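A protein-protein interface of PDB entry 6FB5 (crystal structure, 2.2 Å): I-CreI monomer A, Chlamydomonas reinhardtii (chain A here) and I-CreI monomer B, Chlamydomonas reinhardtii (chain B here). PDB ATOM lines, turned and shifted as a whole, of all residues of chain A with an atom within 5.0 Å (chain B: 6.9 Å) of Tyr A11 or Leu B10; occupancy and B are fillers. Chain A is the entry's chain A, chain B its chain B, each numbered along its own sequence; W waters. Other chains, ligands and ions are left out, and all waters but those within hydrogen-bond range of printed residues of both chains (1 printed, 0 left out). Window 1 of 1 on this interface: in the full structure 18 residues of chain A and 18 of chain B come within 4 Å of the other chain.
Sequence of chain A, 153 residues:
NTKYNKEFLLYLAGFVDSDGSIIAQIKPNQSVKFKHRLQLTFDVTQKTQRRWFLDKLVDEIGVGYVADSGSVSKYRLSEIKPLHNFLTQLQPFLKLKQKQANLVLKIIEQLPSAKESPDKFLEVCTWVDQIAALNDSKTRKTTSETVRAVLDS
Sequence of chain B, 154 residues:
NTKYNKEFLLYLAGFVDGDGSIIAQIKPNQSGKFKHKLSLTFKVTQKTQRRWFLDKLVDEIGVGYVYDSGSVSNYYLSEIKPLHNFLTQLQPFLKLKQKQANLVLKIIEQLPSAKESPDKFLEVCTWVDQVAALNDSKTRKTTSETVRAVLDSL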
ATOM      1  N   GLU A   7     -17.625  -2.741 -26.434  1.00  0.00           N
ATOM      2  CA  GLU A   7     -16.294  -2.199 -26.179  1.00  0.00           C
ATOM      3  C   GLU A   7     -15.539  -1.957 -27.481  1.00  0.00           C
ATOM      4  O   GLU A   7     -14.785  -0.989 -27.602  1.00  0.00           O
ATOM      5  CB  GLU A   7     -15.495  -3.118 -25.256  1.00  0.00           C
ATOM      6  CG  GLU A   7     -16.035  -3.178 -23.838  1.00  0.00           C
ATOM      7  CD  GLU A   7     -15.213  -4.076 -22.938  1.00  0.00           C
ATOM      8  OE1 GLU A   7     -14.277  -4.730 -23.442  1.00  0.00           O
ATOM      9  OE2 GLU A   7     -15.503  -4.128 -21.726  1.00  0.00           O
ATOM     10  N   PHE A   8     -15.747  -2.844 -28.449  1.00  0.00           N
ATOM     11  CA  PHE A   8     -15.182  -2.675 -29.781  1.00  0.00           C
ATOM     12  C   PHE A   8     -15.733  -1.406 -30.422  1.00  0.00           C
ATOM     13  O   PHE A   8     -14.986  -0.613 -30.993  1.00  0.00           O
ATOM     14  CB  PHE A   8     -15.502  -3.892 -30.651  1.00  0.00           C
ATOM     15  CG  PHE A   8     -15.299  -3.661 -32.125  1.00  0.00           C
ATOM     16  CD1 PHE A   8     -14.027  -3.664 -32.673  1.00  0.00           C
ATOM     17  CD2 PHE A   8     -16.384  -3.457 -32.962  1.00  0.00           C
ATOM     18  CE1 PHE A   8     -13.839  -3.458 -34.029  1.00  0.00           C
ATOM     19  CE2 PHE A   8     -16.204  -3.252 -34.317  1.00  0.00           C
ATOM     20  CZ  PHE A   8     -14.930  -3.252 -34.852  1.00  0.00           C
ATOM     21  N   LEU A   9     -17.044  -1.221 -30.309  1.00  0.00           N
ATOM     22  CA  LEU A   9     -17.714  -0.058 -30.884  1.00  0.00           C
ATOM     23  C   LEU A   9     -17.317   1.249 -30.199  1.00  0.00           C
ATOM     24  O   LEU A   9     -17.299   2.303 -30.831  1.00  0.00           O
ATOM     25  CB  LEU A   9     -19.232  -0.236 -30.840  1.00  0.00           C
ATOM     26  CG  LEU A   9     -19.812  -1.282 -31.789  1.00  0.00           C
ATOM     27  CD1 LEU A   9     -21.295  -1.483 -31.526  1.00  0.00           C
ATOM     28  CD2 LEU A   9     -19.579  -0.873 -33.234  1.00  0.00           C
ATOM     29  N   LEU A  10     -17.005   1.178 -28.909  1.00  0.00           N
ATOM     30  CA  LEU A  10     -16.598   2.365 -28.165  1.00  0.00           C
ATOM     31  C   LEU A  10     -15.199   2.829 -28.560  1.00  0.00           C
ATOM     32  O   LEU A  10     -14.972   4.020 -28.770  1.00  0.00           O
ATOM     33  CB  LEU A  10     -16.684   2.129 -26.656  1.00  0.00           C
ATOM     34  CG  LEU A  10     -18.050   2.398 -26.026  1.00  0.00           C
ATOM     35  CD1 LEU A  10     -18.128   1.799 -24.633  1.00  0.00           C
ATOM     36  CD2 LEU A  10     -18.327   3.893 -25.978  1.00  0.00           C
ATOM     37  N   TYR A  11     -14.265   1.888 -28.661  1.00  0.00           N
ATOM     38  CA  TYR A  11     -12.921   2.207 -29.126  1.00  0.00           C
ATOM     39  C   TYR A  11     -12.967   2.696 -30.568  1.00  0.00           C
ATOM     40  O   TYR A  11     -12.341   3.697 -30.914  1.00  0.00           O
ATOM     41  CB  TYR A  11     -11.995   0.990 -29.021  1.00  0.00           C
ATOM     42  CG  TYR A  11     -10.622   1.219 -29.626  1.00  0.00           C
ATOM     43  CD1 TYR A  11     -10.376   0.950 -30.971  1.00  0.00           C
ATOM     44  CD2 TYR A  11      -9.574   1.707 -28.855  1.00  0.00           C
ATOM     45  CE1 TYR A  11      -9.131   1.165 -31.529  1.00  0.00           C
ATOM     46  CE2 TYR A  11      -8.320   1.921 -29.403  1.00  0.00           C
ATOM     47  CZ  TYR A  11      -8.106   1.649 -30.741  1.00  0.00           C
ATOM     48  OH  TYR A  11      -6.863   1.861 -31.292  1.00  0.00           O
ATOM     49  N   LEU A  12     -13.710   1.975 -31.402  1.00  0.00           N
ATOM     50  CA  LEU A  12     -13.783   2.277 -32.826  1.00  0.00           C
ATOM     51  C   LEU A  12     -14.356   3.666 -33.083  1.00  0.00           C
ATOM     52  O   LEU A  12     -13.863   4.392 -33.943  1.00  0.00           O
ATOM     53  CB  LEU A  12     -14.604   1.218 -33.563  1.00  0.00           C
ATOM     54  CG  LEU A  12     -14.679   1.367 -35.081  1.00  0.00           C
ATOM     55  CD1 LEU A  12     -13.282   1.485 -35.671  1.00  0.00           C
ATOM     56  CD2 LEU A  12     -15.423   0.192 -35.693  1.00  0.00           C
ATOM     57  N   ALA A  13     -15.391   4.029 -32.334  1.00  0.00           N
ATOM     58  CA  ALA A  13     -15.994   5.353 -32.453  1.00  0.00           C
ATOM     59  C   ALA A  13     -14.960   6.441 -32.188  1.00  0.00           C
ATOM     60  O   ALA A  13     -14.944   7.472 -32.861  1.00  0.00           O
ATOM     61  CB  ALA A  13     -17.167   5.492 -31.500  1.00  0.00           C
ATOM     62  N   GLY A  14     -14.097   6.205 -31.205  1.00  0.00           N
ATOM     63  CA  GLY A  14     -13.030   7.135 -30.887  1.00  0.00           C
ATOM     64  C   GLY A  14     -12.044   7.275 -32.029  1.00  0.00           C
ATOM     65  O   GLY A  14     -11.644   8.381 -32.390  1.00  0.00           O
ATOM     66  N   PHE A  15     -11.658   6.143 -32.609  1.00  0.00           N
ATOM     67  CA  PHE A  15     -10.687   6.137 -33.693  1.00  0.00           C
ATOM     68  C   PHE A  15     -11.286   6.693 -34.980  1.00  0.00           C
ATOM     69  O   PHE A  15     -10.575   7.250 -35.813  1.00  0.00           O
ATOM     70  CB  PHE A  15     -10.134   4.729 -33.921  1.00  0.00           C
ATOM     71  CG  PHE A  15      -8.822   4.709 -34.648  1.00  0.00           C
ATOM     72  CD1 PHE A  15      -7.639   4.940 -33.967  1.00  0.00           C
ATOM     73  CD2 PHE A  15      -8.768   4.463 -36.009  1.00  0.00           C
ATOM     74  CE1 PHE A  15      -6.426   4.929 -34.629  1.00  0.00           C
ATOM     75  CE2 PHE A  15      -7.559   4.447 -36.678  1.00  0.00           C
ATOM     76  CZ  PHE A  15      -6.386   4.680 -35.986  1.00  0.00           C
ATOM     77  N   PHE A  53      -3.305  -2.746 -38.833  1.00  0.00           N
ATOM     78  CA  PHE A  53      -4.376  -2.259 -37.978  1.00  0.00           C
ATOM     79  C   PHE A  53      -5.670  -2.193 -38.779  1.00  0.00           C
ATOM     80  O   PHE A  53      -6.738  -2.554 -38.286  1.00  0.00           O
ATOM     81  CB  PHE A  53      -4.016  -0.878 -37.428  1.00  0.00           C
ATOM     82  CG  PHE A  53      -4.948  -0.387 -36.358  1.00  0.00           C
ATOM     83  CD1 PHE A  53      -4.792  -0.799 -35.045  1.00  0.00           C
ATOM     84  CD2 PHE A  53      -5.974   0.491 -36.663  1.00  0.00           C
ATOM     85  CE1 PHE A  53      -5.643  -0.347 -34.057  1.00  0.00           C
ATOM     86  CE2 PHE A  53      -6.827   0.949 -35.677  1.00  0.00           C
ATOM     87  CZ  PHE A  53      -6.661   0.529 -34.373  1.00  0.00           C
ATOM     88  N   ASN B   5     -14.264   6.426 -15.673  1.00  0.00           N
ATOM     89  CA  ASN B   5     -15.221   5.457 -16.188  1.00  0.00           C
ATOM     90  C   ASN B   5     -14.648   4.677 -17.365  1.00  0.00           C
ATOM     91  O   ASN B   5     -13.892   5.221 -18.170  1.00  0.00           O
ATOM     92  CB  ASN B   5     -16.530   6.142 -16.589  1.00  0.00           C
ATOM     93  CG  ASN B   5     -17.316   6.643 -15.394  1.00  0.00           C
ATOM     94  OD1 ASN B   5     -17.186   6.120 -14.288  1.00  0.00           O
ATOM     95  ND2 ASN B   5     -18.141   7.660 -15.613  1.00  0.00           N
ATOM     96  N   LYS B   6     -15.015   3.404 -17.454  1.00  0.00           N
ATOM     97  CA  LYS B   6     -14.462   2.509 -18.464  1.00  0.00           C
ATOM     98  C   LYS B   6     -14.842   2.913 -19.886  1.00  0.00           C
ATOM     99  O   LYS B   6     -13.995   2.937 -20.777  1.00  0.00           O
ATOM    100  CB  LYS B   6     -14.917   1.074 -18.197  1.00  0.00           C
ATOM    101  CG  LYS B   6     -14.319   0.053 -19.145  1.00  0.00           C
ATOM    102  CD  LYS B   6     -14.883  -1.330 -18.876  1.00  0.00           C
ATOM    103  CE  LYS B   6     -14.010  -2.408 -19.488  1.00  0.00           C
ATOM    104  NZ  LYS B   6     -14.547  -3.769 -19.217  1.00  0.00           N
ATOM    105  N   GLU B   7     -16.119   3.222 -20.093  1.00  0.00           N
ATOM    106  CA  GLU B   7     -16.609   3.592 -21.417  1.00  0.00           C
ATOM    107  C   GLU B   7     -15.956   4.880 -21.906  1.00  0.00           C
ATOM    108  O   GLU B   7     -15.757   5.073 -23.105  1.00  0.00           O
ATOM    109  CB  GLU B   7     -18.132   3.730 -21.414  1.00  0.00           C
ATOM    110  CG  GLU B   7     -18.862   2.431 -21.115  1.00  0.00           C
ATOM    111  CD  GLU B   7     -20.352   2.520 -21.384  1.00  0.00           C
ATOM    112  OE1 GLU B   7     -20.860   3.646 -21.561  1.00  0.00           O
ATOM    113  OE2 GLU B   7     -21.012   1.462 -21.427  1.00  0.00           O
ATOM    114  N   PHE B   8     -15.624   5.757 -20.964  1.00  0.00           N
ATOM    115  CA  PHE B   8     -14.899   6.982 -21.267  1.00  0.00           C
ATOM    116  C   PHE B   8     -13.477   6.659 -21.714  1.00  0.00           C
ATOM    117  O   PHE B   8     -12.982   7.222 -22.689  1.00  0.00           O
ATOM    118  CB  PHE B   8     -14.881   7.900 -20.043  1.00  0.00           C
ATOM    119  CG  PHE B   8     -13.816   8.959 -20.089  1.00  0.00           C
ATOM    120  CD1 PHE B   8     -13.977  10.093 -20.868  1.00  0.00           C
ATOM    121  CD2 PHE B   8     -12.657   8.827 -19.339  1.00  0.00           C
ATOM    122  CE1 PHE B   8     -12.999  11.069 -20.908  1.00  0.00           C
ATOM    123  CE2 PHE B   8     -11.677   9.801 -19.373  1.00  0.00           C
ATOM    124  CZ  PHE B   8     -11.849  10.924 -20.157  1.00  0.00           C
ATOM    125  N   LEU B   9     -12.830   5.744 -20.999  1.00  0.00           N
ATOM    126  CA  LEU B   9     -11.467   5.334 -21.326  1.00  0.00           C
ATOM    127  C   LEU B   9     -11.383   4.602 -22.663  1.00  0.00           C
ATOM    128  O   LEU B   9     -10.407   4.749 -23.397  1.00  0.00           O
ATOM    129  CB  LEU B   9     -10.884   4.458 -20.214  1.00  0.00           C
ATOM    130  CG  LEU B   9     -10.536   5.159 -18.900  1.00  0.00           C
ATOM    131  CD1 LEU B   9     -10.088   4.153 -17.852  1.00  0.00           C
ATOM    132  CD2 LEU B   9      -9.458   6.206 -19.130  1.00  0.00           C
ATOM    133  N   LEU B  10     -12.407   3.811 -22.972  1.00  0.00           N
ATOM    134  CA  LEU B  10     -12.443   3.044 -24.216  1.00  0.00           C
ATOM    135  C   LEU B  10     -12.554   3.947 -25.443  1.00  0.00           C
ATOM    136  O   LEU B  10     -11.829   3.767 -26.421  1.00  0.00           O
ATOM    137  CB  LEU B  10     -13.591   2.032 -24.191  1.00  0.00           C
ATOM    138  CG  LEU B  10     -13.303   0.716 -23.469  1.00  0.00           C
ATOM    139  CD1 LEU B  10     -14.585   0.110 -22.925  1.00  0.00           C
ATOM    140  CD2 LEU B  10     -12.614  -0.256 -24.412  1.00  0.00           C
ATOM    141  N   TYR B  11     -13.464   4.916 -25.389  1.00  0.00           N
ATOM    142  CA  TYR B  11     -13.613   5.874 -26.478  1.00  0.00           C
ATOM    143  C   TYR B  11     -12.361   6.727 -26.620  1.00  0.00           C
ATOM    144  O   TYR B  11     -11.856   6.928 -27.723  1.00  0.00           O
ATOM    145  CB  TYR B  11     -14.829   6.781 -26.256  1.00  0.00           C
ATOM    146  CG  TYR B  11     -14.929   7.910 -27.261  1.00  0.00           C
ATOM    147  CD1 TYR B  11     -15.605   7.739 -28.461  1.00  0.00           C
ATOM    148  CD2 TYR B  11     -14.341   9.147 -27.010  1.00  0.00           C
ATOM    149  CE1 TYR B  11     -15.694   8.767 -29.384  1.00  0.00           C
ATOM    150  CE2 TYR B  11     -14.419  10.174 -27.927  1.00  0.00           C
ATOM    151  CZ  TYR B  11     -15.097   9.981 -29.111  1.00  0.00           C
ATOM    152  OH  TYR B  11     -15.177  11.009 -30.022  1.00  0.00           O
ATOM    153  N   LEU B  12     -11.876   7.236 -25.492  1.00  0.00           N
ATOM    154  CA  LEU B  12     -10.730   8.136 -25.481  1.00  0.00           C
ATOM    155  C   LEU B  12      -9.481   7.464 -26.034  1.00  0.00           C
ATOM    156  O   LEU B  12      -8.688   8.094 -26.729  1.00  0.00           O
ATOM    157  CB  LEU B  12     -10.471   8.661 -24.068  1.00  0.00           C
ATOM    158  CG  LEU B  12      -9.322   9.651 -23.891  1.00  0.00           C
ATOM    159  CD1 LEU B  12      -9.509  10.871 -24.784  1.00  0.00           C
ATOM    160  CD2 LEU B  12      -9.203  10.066 -22.437  1.00  0.00           C
ATOM    161  N   ALA B  13      -9.315   6.181 -25.725  1.00  0.00           N
ATOM    162  CA  ALA B  13      -8.177   5.414 -26.219  1.00  0.00           C
ATOM    163  C   ALA B  13      -8.160   5.392 -27.743  1.00  0.00           C
ATOM    164  O   ALA B  13      -7.113   5.576 -28.363  1.00  0.00           O
ATOM    165  CB  ALA B  13      -8.209   4.000 -25.667  1.00  0.00           C
ATOM    166  N   GLY B  14      -9.326   5.166 -28.338  1.00  0.00           N
ATOM    167  CA  GLY B  14      -9.459   5.169 -29.782  1.00  0.00           C
ATOM    168  C   GLY B  14      -9.144   6.530 -30.368  1.00  0.00           C
ATOM    169  O   GLY B  14      -8.478   6.639 -31.398  1.00  0.00           O
ATOM    170  N   PHE B  15      -9.616   7.575 -29.699  1.00  0.00           N
ATOM    171  CA  PHE B  15      -9.390   8.937 -30.164  1.00  0.00           C
ATOM    172  C   PHE B  15      -7.929   9.346 -30.001  1.00  0.00           C
ATOM    173  O   PHE B  15      -7.397  10.109 -30.806  1.00  0.00           O
ATOM    174  CB  PHE B  15     -10.305   9.918 -29.432  1.00  0.00           C
ATOM    175  CG  PHE B  15     -10.468  11.233 -30.139  1.00  0.00           C
ATOM    176  CD1 PHE B  15     -11.474  11.409 -31.073  1.00  0.00           C
ATOM    177  CD2 PHE B  15      -9.614  12.290 -29.874  1.00  0.00           C
ATOM    178  CE1 PHE B  15     -11.631  12.617 -31.727  1.00  0.00           C
ATOM    179  CE2 PHE B  15      -9.762  13.499 -30.526  1.00  0.00           C
ATOM    180  CZ  PHE B  15     -10.772  13.664 -31.453  1.00  0.00           C
ATOM    181  N   ASP B  17      -5.326   7.117 -30.010  1.00  0.00           N
ATOM    182  CA  ASP B  17      -4.605   6.344 -31.020  1.00  0.00           C
ATOM    183  C   ASP B  17      -4.679   7.014 -32.391  1.00  0.00           C
ATOM    184  O   ASP B  17      -3.803   6.823 -33.234  1.00  0.00           O
ATOM    185  CB  ASP B  17      -5.144   4.913 -31.104  1.00  0.00           C
ATOM    186  CG  ASP B  17      -4.512   3.988 -30.082  1.00  0.00           C
ATOM    187  OD1 ASP B  17      -3.409   4.308 -29.591  1.00  0.00           O
ATOM    188  OD2 ASP B  17      -5.112   2.937 -29.777  1.00  0.00           O
ATOM    189  N   GLY B  18      -5.726   7.810 -32.597  1.00  0.00           N
ATOM    190  CA  GLY B  18      -5.942   8.495 -33.859  1.00  0.00           C
ATOM    191  C   GLY B  18      -5.379   9.905 -33.938  1.00  0.00           C
ATOM    192  O   GLY B  18      -4.462  10.167 -34.717  1.00  0.00           O
ATOM    193  N   LEU B  90      -5.536   4.388 -18.838  1.00  0.00           N
ATOM    194  CA  LEU B  90      -5.788   4.451 -20.275  1.00  0.00           C
ATOM    195  C   LEU B  90      -5.067   3.334 -21.021  1.00  0.00           C
ATOM    196  O   LEU B  90      -5.596   2.772 -21.979  1.00  0.00           O
ATOM    197  CB  LEU B  90      -5.357   5.806 -20.836  1.00  0.00           C
ATOM    198  CG  LEU B  90      -5.604   6.028 -22.328  1.00  0.00           C
ATOM    199  CD1 LEU B  90      -7.095   6.137 -22.611  1.00  0.00           C
ATOM    200  CD2 LEU B  90      -4.869   7.262 -22.821  1.00  0.00           C
ATOM    201  N   PRO B  92      -4.453   0.070 -20.760  1.00  0.00           N
ATOM    202  CA  PRO B  92      -5.032  -1.220 -21.170  1.00  0.00           C
ATOM    203  C   PRO B  92      -5.914  -1.137 -22.416  1.00  0.00           C
ATOM    204  O   PRO B  92      -6.216  -2.169 -23.017  1.00  0.00           O
ATOM    205  CB  PRO B  92      -5.890  -1.615 -19.962  1.00  0.00           C
ATOM    206  CG  PRO B  92      -5.274  -0.911 -18.814  1.00  0.00           C
ATOM    207  CD  PRO B  92      -4.795   0.395 -19.363  1.00  0.00           C
ATOM    208  N   PHE B  93      -6.315   0.068 -22.802  1.00  0.00           N
ATOM    209  CA  PHE B  93      -7.260   0.230 -23.899  1.00  0.00           C
ATOM    210  C   PHE B  93      -6.627   0.791 -25.171  1.00  0.00           C
ATOM    211  O   PHE B  93      -7.255   0.811 -26.228  1.00  0.00           O
ATOM    212  CB  PHE B  93      -8.438   1.095 -23.449  1.00  0.00           C
ATOM    213  CG  PHE B  93      -9.097   0.605 -22.193  1.00  0.00           C
ATOM    214  CD1 PHE B  93      -9.912  -0.514 -22.217  1.00  0.00           C
ATOM    215  CD2 PHE B  93      -8.893   1.254 -20.988  1.00  0.00           C
ATOM    216  CE1 PHE B  93     -10.518  -0.974 -21.064  1.00  0.00           C
ATOM    217  CE2 PHE B  93      -9.498   0.799 -19.828  1.00  0.00           C
ATOM    218  CZ  PHE B  93     -10.312  -0.317 -19.868  1.00  0.00           C
ATOM    219  N   LEU B  94      -5.380   1.240 -25.068  1.00  0.00           N
ATOM    220  CA  LEU B  94      -4.653   1.733 -26.232  1.00  0.00           C
ATOM    221  C   LEU B  94      -4.225   0.573 -27.122  1.00  0.00           C
ATOM    222  O   LEU B  94      -3.886  -0.503 -26.629  1.00  0.00           O
ATOM    223  CB  LEU B  94      -3.427   2.536 -25.795  1.00  0.00           C
ATOM    224  CG  LEU B  94      -3.701   3.818 -25.009  1.00  0.00           C
ATOM    225  CD1 LEU B  94      -2.434   4.311 -24.343  1.00  0.00           C
ATOM    226  CD2 LEU B  94      -4.274   4.891 -25.925  1.00  0.00           C
ATOM    227  N   LYS B  95      -4.242   0.792 -28.431  1.00  0.00           N
ATOM    228  CA  LYS B  95      -3.827  -0.241 -29.374  1.00  0.00           C
ATOM    229  C   LYS B  95      -2.567   0.157 -30.135  1.00  0.00           C
ATOM    230  O   LYS B  95      -1.643  -0.641 -30.276  1.00  0.00           O
ATOM    231  CB  LYS B  95      -4.955  -0.568 -30.356  1.00  0.00           C
ATOM    232  CG  LYS B  95      -6.160  -1.234 -29.717  1.00  0.00           C
ATOM    233  CD  LYS B  95      -7.135  -1.724 -30.771  1.00  0.00           C
ATOM    234  CE  LYS B  95      -8.252  -2.550 -30.153  1.00  0.00           C
ATOM    235  NZ  LYS B  95      -9.118  -1.737 -29.254  1.00  0.00           N
ATOM    236  N   LEU B  96      -2.533   1.391 -30.626  1.00  0.00           N
ATOM    237  CA  LEU B  96      -1.392   1.868 -31.400  1.00  0.00           C
ATOM    238  C   LEU B  96      -0.295   2.465 -30.526  1.00  0.00           C
ATOM    239  O   LEU B  96       0.884   2.402 -30.870  1.00  0.00           O
ATOM    240  CB  LEU B  96      -1.836   2.898 -32.438  1.00  0.00           C
ATOM    241  CG  LEU B  96      -2.700   2.391 -33.589  1.00  0.00           C
ATOM    242  CD1 LEU B  96      -3.008   3.525 -34.559  1.00  0.00           C
ATOM    243  CD2 LEU B  96      -2.013   1.240 -34.305  1.00  0.00           C
ATOM    244  N   LYS B  97      -0.684   3.046 -29.397  1.00  0.00           N
ATOM    245  CA  LYS B  97       0.256   3.795 -28.573  1.00  0.00           C
ATOM    246  C   LYS B  97       0.435   3.206 -27.180  1.00  0.00           C
ATOM    247  O   LYS B  97       0.868   3.898 -26.259  1.00  0.00           O
ATOM    248  CB  LYS B  97      -0.188   5.255 -28.471  1.00  0.00           C
ATOM    249  CG  LYS B  97      -0.243   5.972 -29.808  1.00  0.00           C
ATOM    250  CD  LYS B  97      -0.989   7.290 -29.700  1.00  0.00           C
ATOM    251  CE  LYS B  97      -1.006   8.020 -31.029  1.00  0.00           C
ATOM    252  NZ  LYS B  97       0.357   8.447 -31.442  1.00  0.00           N
HETATM  253  O   HOH W   1     -11.795  -2.245 -27.220  1.00  0.00           O
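Tyr A11 touches six residues of chain B. Printed residues of chain B within 4 Å of Phe A15: Gly B14 (3.2 Å), Phe B15 (3.8 Å), Asp B17 (3.5 Å), Gly B18 (3.6 Å) and Leu B96 (3.7 Å). Printed residues of chain A within 4 Å of Lys B6: Glu A7 (2.7 Å). Of chain A, only Glu A7, Leu A10 and Tyr A11 come within 4 Å of Leu B10. Leu B12 touches none of the printed residues of chain A. The nearest printed residue of chain A that does not touch Leu B10 is Leu A12 (5.6 Å).
The backbone NH (N) of Leu B96 lies within hydrogen-bond range of the side-chain carboxylate (OD2) of Asp B17 (3.1 Å). N of Lys B97 sits at hydrogen-bond distance from OD1 of Asp B17, at 3.0 Å. The side-chain carboxylate of Asp B17 lies within hydrogen-bond range of the backbone NH of Lys B95, at 2.7 Å.
The side-chain carboxylate of Asp B17 is in hydrogen-bond range of the side-chain hydroxyl of Tyr A11 (2.6 Å). The side-chain amino group (NZ) of Lys B6 lies within salt-bridge range of the side-chain carboxylate (OE2) of Glu A7 (2.7 Å). N of Phe A15 sits close to O of Gly B14, 3.4 Å away. O of Gly A14 sits close to N of Phe B15, at 3.5 Å.
Water W1 lies within hydrogen-bond range of O of Glu A7 (3.3 Å) and NZ of Lys B95 (3.4 Å).
Of the 20 printed residues of chain B, 12 touch a printed residue of chain A. Hydrophobic or aromatic side chains of chain B within 4 Å of the printed part of chain A: Leu B10, Tyr B11, Phe B15 and Leu B96. Of the 10 printed residues of chain A, 7 touch a printed residue of chain B. Among the printed residues, 22 pairs touch across the chains. Among the printed residues, Asp or Glu carboxylates within 4 Å of a Lys or Arg side-chain nitrogen of the other chain: Glu A7 with Lys B6.
Among the printed residues, merely in contact across the chains: Tyr A11 with Lys B95 (3.2 Å), Leu A10 with Tyr B11 (3.2 Å), Tyr A11 with Leu B10 (3.3 Å), Gly A14 with Tyr B11 (3.4 Å), Gly A14 with Gly B14 (3.4 Å), Tyr A11 with Gly B14 (3.4 Å), Phe A15 with Asp B17 (3.5 Å), Phe A53 with Leu B96 (3.5 Å), Tyr A11 with Phe B93 (3.5 Å), Phe A15 with Gly B18 (3.6 Å), Leu A10 with Glu B7 (3.6 Å), Phe A15 with Leu B96 (3.7 Å), Glu A7 with Leu B10 (3.7 Å), Ala A13 with Tyr B11 (3.7 Å), Phe A53 with Lys B95 (3.8 Å), Phe A15 with Phe B15 (3.8 Å), Tyr A11 with Ala B13 (3.9 Å) and Leu A10 with Leu B10 (3.9 Å).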
